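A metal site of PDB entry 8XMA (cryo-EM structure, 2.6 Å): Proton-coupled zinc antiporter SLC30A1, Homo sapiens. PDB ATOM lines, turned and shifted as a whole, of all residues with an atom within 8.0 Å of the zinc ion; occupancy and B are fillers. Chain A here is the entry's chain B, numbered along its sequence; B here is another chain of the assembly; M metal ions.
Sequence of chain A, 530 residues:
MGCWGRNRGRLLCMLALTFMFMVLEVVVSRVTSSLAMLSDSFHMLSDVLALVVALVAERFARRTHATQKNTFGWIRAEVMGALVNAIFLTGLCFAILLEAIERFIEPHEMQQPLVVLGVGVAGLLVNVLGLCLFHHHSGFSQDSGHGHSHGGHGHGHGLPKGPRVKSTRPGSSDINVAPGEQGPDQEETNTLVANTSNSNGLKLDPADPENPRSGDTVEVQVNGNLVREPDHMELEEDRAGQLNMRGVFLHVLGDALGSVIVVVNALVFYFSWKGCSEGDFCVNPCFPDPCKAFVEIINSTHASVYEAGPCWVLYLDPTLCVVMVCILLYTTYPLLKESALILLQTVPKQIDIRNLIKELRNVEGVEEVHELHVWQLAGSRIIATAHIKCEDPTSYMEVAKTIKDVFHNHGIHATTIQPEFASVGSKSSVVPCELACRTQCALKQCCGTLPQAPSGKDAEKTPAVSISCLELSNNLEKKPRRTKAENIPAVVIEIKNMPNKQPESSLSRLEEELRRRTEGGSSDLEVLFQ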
ATOM      1  N   GLU A 368     -22.550 -11.928   6.298  1.00  0.00           N
ATOM      2  CA  GLU A 368     -22.403 -12.457   4.954  1.00  0.00           C
ATOM      3  C   GLU A 368     -20.956 -12.274   4.519  1.00  0.00           C
ATOM      4  O   GLU A 368     -20.277 -11.346   4.947  1.00  0.00           O
ATOM      5  CB  GLU A 368     -23.369 -11.779   3.969  1.00  0.00           C
ATOM      6  CG  GLU A 368     -23.177 -10.281   3.790  1.00  0.00           C
ATOM      7  CD  GLU A 368     -22.126  -9.935   2.748  1.00  0.00           C
ATOM      8  OE1 GLU A 368     -21.821 -10.811   1.912  1.00  0.00           O
ATOM      9  OE2 GLU A 368     -21.614  -8.805   2.778  1.00  0.00           O
ATOM     10  N   VAL A 369     -20.494 -13.186   3.656  1.00  0.00           N
ATOM     11  CA  VAL A 369     -19.130 -13.180   3.164  1.00  0.00           C
ATOM     12  C   VAL A 369     -19.155 -13.038   1.648  1.00  0.00           C
ATOM     13  O   VAL A 369     -19.804 -13.823   0.963  1.00  0.00           O
ATOM     14  CB  VAL A 369     -18.375 -14.461   3.574  1.00  0.00           C
ATOM     15  CG1 VAL A 369     -16.987 -14.476   2.945  1.00  0.00           C
ATOM     16  CG2 VAL A 369     -18.287 -14.566   5.091  1.00  0.00           C
ATOM     17  N   HIS A 370     -18.446 -12.027   1.141  1.00  0.00           N
ATOM     18  CA  HIS A 370     -18.365 -11.794  -0.296  1.00  0.00           C
ATOM     19  C   HIS A 370     -16.940 -11.433  -0.665  1.00  0.00           C
ATOM     20  O   HIS A 370     -16.127 -11.065   0.190  1.00  0.00           O
ATOM     21  CB  HIS A 370     -19.333 -10.679  -0.736  1.00  0.00           C
ATOM     22  CG  HIS A 370     -18.932  -9.323  -0.269  1.00  0.00           C
ATOM     23  ND1 HIS A 370     -19.188  -8.869   1.001  1.00  0.00           N
ATOM     24  CD2 HIS A 370     -18.312  -8.305  -0.917  1.00  0.00           C
ATOM     25  CE1 HIS A 370     -18.731  -7.635   1.130  1.00  0.00           C
ATOM     26  NE2 HIS A 370     -18.192  -7.267  -0.021  1.00  0.00           N
ATOM     27  N   GLU A 371     -16.630 -11.565  -1.950  1.00  0.00           N
ATOM     28  CA  GLU A 371     -15.296 -11.316  -2.491  1.00  0.00           C
ATOM     29  C   GLU A 371     -14.258 -12.212  -1.809  1.00  0.00           C
ATOM     30  O   GLU A 371     -13.272 -11.752  -1.240  1.00  0.00           O
ATOM     31  CB  GLU A 371     -14.930  -9.833  -2.363  1.00  0.00           C
ATOM     32  CG  GLU A 371     -13.763  -9.399  -3.233  1.00  0.00           C
ATOM     33  CD  GLU A 371     -14.158  -9.218  -4.681  1.00  0.00           C
ATOM     34  OE1 GLU A 371     -15.322  -8.850  -4.946  1.00  0.00           O
ATOM     35  OE2 GLU A 371     -13.301  -9.445  -5.564  1.00  0.00           O
ATOM     36  N   LEU A 372     -14.522 -13.512  -1.871  1.00  0.00           N
ATOM     37  CA  LEU A 372     -13.606 -14.513  -1.322  1.00  0.00           C
ATOM     38  C   LEU A 372     -12.649 -14.964  -2.415  1.00  0.00           C
ATOM     39  O   LEU A 372     -13.072 -15.514  -3.432  1.00  0.00           O
ATOM     40  CB  LEU A 372     -14.376 -15.717  -0.768  1.00  0.00           C
ATOM     41  CG  LEU A 372     -13.482 -16.826  -0.216  1.00  0.00           C
ATOM     42  CD1 LEU A 372     -13.013 -16.497   1.183  1.00  0.00           C
ATOM     43  CD2 LEU A 372     -14.201 -18.165  -0.242  1.00  0.00           C
ATOM     44  N   ALA A 386     -11.009 -12.106   1.927  1.00  0.00           N
ATOM     45  CA  ALA A 386     -12.465 -12.044   1.958  1.00  0.00           C
ATOM     46  C   ALA A 386     -12.923 -10.736   2.576  1.00  0.00           C
ATOM     47  O   ALA A 386     -12.190 -10.078   3.322  1.00  0.00           O
ATOM     48  CB  ALA A 386     -13.050 -13.228   2.739  1.00  0.00           C
ATOM     49  N   HIS A 387     -14.153 -10.361   2.256  1.00  0.00           N
ATOM     50  CA  HIS A 387     -14.829  -9.216   2.853  1.00  0.00           C
ATOM     51  C   HIS A 387     -15.999  -9.726   3.690  1.00  0.00           C
ATOM     52  O   HIS A 387     -16.728 -10.633   3.260  1.00  0.00           O
ATOM     53  CB  HIS A 387     -15.341  -8.245   1.786  1.00  0.00           C
ATOM     54  CG  HIS A 387     -14.263  -7.642   0.945  1.00  0.00           C
ATOM     55  ND1 HIS A 387     -14.490  -6.575   0.099  1.00  0.00           N
ATOM     56  CD2 HIS A 387     -12.951  -7.964   0.802  1.00  0.00           C
ATOM     57  CE1 HIS A 387     -13.368  -6.269  -0.518  1.00  0.00           C
ATOM     58  NE2 HIS A 387     -12.422  -7.094  -0.115  1.00  0.00           N
ATOM     59  N   ILE A 388     -16.183  -9.151   4.871  1.00  0.00           N
ATOM     60  CA  ILE A 388     -17.233  -9.596   5.780  1.00  0.00           C
ATOM     61  C   ILE A 388     -18.017  -8.389   6.263  1.00  0.00           C
ATOM     62  O   ILE A 388     -17.531  -7.250   6.238  1.00  0.00           O
ATOM     63  CB  ILE A 388     -16.666 -10.370   6.990  1.00  0.00           C
ATOM     64  CG1 ILE A 388     -15.653  -9.519   7.735  1.00  0.00           C
ATOM     65  CG2 ILE A 388     -16.037 -11.684   6.527  1.00  0.00           C
ATOM     66  CD1 ILE A 388     -15.257 -10.081   9.082  1.00  0.00           C
ATOM     67  N   LYS A 389     -19.251  -8.629   6.702  1.00  0.00           N
ATOM     68  CA  LYS A 389     -20.087  -7.636   7.344  1.00  0.00           C
ATOM     69  C   LYS A 389     -20.384  -8.091   8.760  1.00  0.00           C
ATOM     70  O   LYS A 389     -20.892  -9.205   8.960  1.00  0.00           O
ATOM     71  CB  LYS A 389     -21.379  -7.410   6.566  1.00  0.00           C
ATOM     72  CG  LYS A 389     -21.198  -6.647   5.258  1.00  0.00           C
ATOM     73  CD  LYS A 389     -22.532  -6.364   4.605  1.00  0.00           C
ATOM     74  CE  LYS A 389     -22.357  -5.661   3.267  1.00  0.00           C
ATOM     75  NZ  LYS A 389     -21.856  -4.266   3.436  1.00  0.00           N
ATOM     76  N   GLN A 418     -11.353  -8.122   5.409  1.00  0.00           N
ATOM     77  CA  GLN A 418     -11.725  -6.711   5.512  1.00  0.00           C
ATOM     78  C   GLN A 418     -13.153  -6.593   5.992  1.00  0.00           C
ATOM     79  O   GLN A 418     -14.078  -6.976   5.260  1.00  0.00           O
ATOM     80  CB  GLN A 418     -11.551  -6.018   4.165  1.00  0.00           C
ATOM     81  CG  GLN A 418     -12.235  -4.666   4.077  1.00  0.00           C
ATOM     82  CD  GLN A 418     -12.498  -4.235   2.652  1.00  0.00           C
ATOM     83  OE1 GLN A 418     -11.581  -4.167   1.842  1.00  0.00           O
ATOM     84  NE2 GLN A 418     -13.752  -3.941   2.349  1.00  0.00           N
ATOM     85  N   PRO A 419     -13.398  -6.077   7.197  1.00  0.00           N
ATOM     86  CA  PRO A 419     -14.772  -5.910   7.667  1.00  0.00           C
ATOM     87  C   PRO A 419     -15.454  -4.738   6.973  1.00  0.00           C
ATOM     88  O   PRO A 419     -14.808  -3.799   6.494  1.00  0.00           O
ATOM     89  CB  PRO A 419     -14.615  -5.636   9.167  1.00  0.00           C
ATOM     90  CG  PRO A 419     -13.161  -5.844   9.473  1.00  0.00           C
ATOM     91  CD  PRO A 419     -12.422  -5.650   8.201  1.00  0.00           C
ATOM     92  N   GLU A 420     -16.777  -4.805   6.924  1.00  0.00           N
ATOM     93  CA  GLU A 420     -17.604  -3.708   6.441  1.00  0.00           C
ATOM     94  C   GLU A 420     -18.773  -3.528   7.398  1.00  0.00           C
ATOM     95  O   GLU A 420     -19.401  -4.512   7.808  1.00  0.00           O
ATOM     96  CB  GLU A 420     -18.116  -3.962   5.026  1.00  0.00           C
ATOM     97  CG  GLU A 420     -17.018  -4.288   4.019  1.00  0.00           C
ATOM     98  CD  GLU A 420     -17.572  -4.731   2.674  1.00  0.00           C
ATOM     99  OE1 GLU A 420     -18.769  -4.505   2.419  1.00  0.00           O
ATOM    100  OE2 GLU A 420     -16.797  -5.299   1.883  1.00  0.00           O
ATOM    101  N   PRO A 432     -23.782  -4.272  -2.779  1.00  0.00           N
ATOM    102  CA  PRO A 432     -23.121  -5.533  -2.421  1.00  0.00           C
ATOM    103  C   PRO A 432     -21.872  -5.330  -1.572  1.00  0.00           C
ATOM    104  O   PRO A 432     -21.608  -6.132  -0.668  1.00  0.00           O
ATOM    105  CB  PRO A 432     -22.804  -6.171  -3.781  1.00  0.00           C
ATOM    106  CG  PRO A 432     -22.754  -5.016  -4.726  1.00  0.00           C
ATOM    107  CD  PRO A 432     -23.778  -4.043  -4.238  1.00  0.00           C
ATOM    108  N   CYS A 433     -21.105  -4.284  -1.859  1.00  0.00           N
ATOM    109  CA  CYS A 433     -19.869  -4.011  -1.131  1.00  0.00           C
ATOM    110  C   CYS A 433     -19.745  -2.519  -0.858  1.00  0.00           C
ATOM    111  O   CYS A 433     -19.650  -1.725  -1.799  1.00  0.00           O
ATOM    112  CB  CYS A 433     -18.657  -4.517  -1.915  1.00  0.00           C
ATOM    113  SG  CYS A 433     -17.057  -4.302  -1.092  1.00  0.00           S
ATOM    114  N   GLU A 434     -19.743  -2.136   0.411  1.00  0.00           N
ATOM    115  CA  GLU A 434     -19.671  -0.710   0.763  1.00  0.00           C
ATOM    116  C   GLU A 434     -18.374  -0.047   0.326  1.00  0.00           C
ATOM    117  O   GLU A 434     -18.394   1.090  -0.163  1.00  0.00           O
ATOM    118  CB  GLU A 434     -19.857  -0.537   2.267  1.00  0.00           C
ATOM    119  CG  GLU A 434     -21.248  -0.872   2.744  1.00  0.00           C
ATOM    120  CD  GLU A 434     -21.267  -1.245   4.211  1.00  0.00           C
ATOM    121  OE1 GLU A 434     -20.174  -1.358   4.803  1.00  0.00           O
ATOM    122  OE2 GLU A 434     -22.370  -1.440   4.761  1.00  0.00           O
ATOM    123  N   LEU A 435     -17.252  -0.736   0.490  1.00  0.00           N
ATOM    124  CA  LEU A 435     -15.982  -0.174   0.050  1.00  0.00           C
ATOM    125  C   LEU A 435     -15.782  -0.453  -1.430  1.00  0.00           C
ATOM    126  O   LEU A 435     -15.039  -1.356  -1.807  1.00  0.00           O
ATOM    127  CB  LEU A 435     -14.820  -0.762   0.850  1.00  0.00           C
ATOM    128  CG  LEU A 435     -14.434  -0.006   2.123  1.00  0.00           C
ATOM    129  CD1 LEU A 435     -13.114  -0.532   2.651  1.00  0.00           C
ATOM    130  CD2 LEU A 435     -14.321   1.473   1.818  1.00  0.00           C
ATOM    131  N   ALA A 436     -16.441   0.344  -2.275  1.00  0.00           N
ATOM    132  CA  ALA A 436     -16.342   0.113  -3.712  1.00  0.00           C
ATOM    133  C   ALA A 436     -15.739   1.338  -4.374  1.00  0.00           C
ATOM    134  O   ALA A 436     -15.803   2.460  -3.854  1.00  0.00           O
ATOM    135  CB  ALA A 436     -17.711  -0.196  -4.322  1.00  0.00           C
ATOM    136  N   LYS B 404      -9.201   3.635   0.766  1.00  0.00           N
ATOM    137  CA  LYS B 404      -9.732   3.293  -0.555  1.00  0.00           C
ATOM    138  C   LYS B 404      -9.470   4.405  -1.552  1.00  0.00           C
ATOM    139  O   LYS B 404      -9.105   4.158  -2.699  1.00  0.00           O
ATOM    140  CB  LYS B 404     -11.218   2.984  -0.463  1.00  0.00           C
ATOM    141  CG  LYS B 404     -11.853   2.574  -1.784  1.00  0.00           C
ATOM    142  CD  LYS B 404     -11.285   1.281  -2.328  1.00  0.00           C
ATOM    143  CE  LYS B 404     -11.706   0.102  -1.475  1.00  0.00           C
ATOM    144  NZ  LYS B 404     -11.213  -1.184  -2.031  1.00  0.00           N
ATOM    145  N   THR B 415      -9.045  -3.711  -3.758  1.00  0.00           N
ATOM    146  CA  THR B 415      -8.217  -3.722  -2.568  1.00  0.00           C
ATOM    147  C   THR B 415      -8.893  -4.519  -1.448  1.00  0.00           C
ATOM    148  O   THR B 415     -10.049  -4.930  -1.549  1.00  0.00           O
ATOM    149  CB  THR B 415      -7.933  -2.295  -2.088  1.00  0.00           C
ATOM    150  OG1 THR B 415      -9.097  -1.762  -1.444  1.00  0.00           O
ATOM    151  CG2 THR B 415      -7.575  -1.411  -3.260  1.00  0.00           C
ATOM    152  N   THR B 416      -8.122  -4.732  -0.387  1.00  0.00           N
ATOM    153  CA  THR B 416      -8.631  -5.386   0.816  1.00  0.00           C
ATOM    154  C   THR B 416      -7.760  -4.948   1.986  1.00  0.00           C
ATOM    155  O   THR B 416      -6.575  -5.287   2.031  1.00  0.00           O
ATOM    156  CB  THR B 416      -8.617  -6.902   0.673  1.00  0.00           C
ATOM    157  OG1 THR B 416      -9.497  -7.298  -0.385  1.00  0.00           O
ATOM    158  CG2 THR B 416      -9.074  -7.558   1.969  1.00  0.00           C
HETATM  159 ZN    ZN M   1     -16.479  -6.212   0.149  1.00  0.00          ZN
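SG of Cys 433 lies close to O of Leu 435 (3.6 Å).
O of Ile 388 sits at hydrogen-bond distance from N of Glu 420 (2.6 Å).
OE2 of Glu 420 lies close to NE2 of Gln 418 (3.4 Å).
NZ of Lys 389 is in salt-bridge range of OE1 of Glu 420 (3.3 Å).
NE2 of His 387 lies within hydrogen-bond range of OG1 of Thr 416 of chain B, 2.9 Å away.
OE1 of Glu 420 sits at hydrogen-bond distance from N of Glu 434, 3.3 Å away.
A ring nitrogen (ND1) of His 370 lies within hydrogen-bond range of the side-chain carboxylate (OE2) of Glu 368.
The zinc ion is bound by OE2 of Glu 420 (2.0 Å), NE2 of His 370 (2.0 Å), ND1 of His 387 (2.0 Å) and SG of Cys 433 (2.3 Å).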
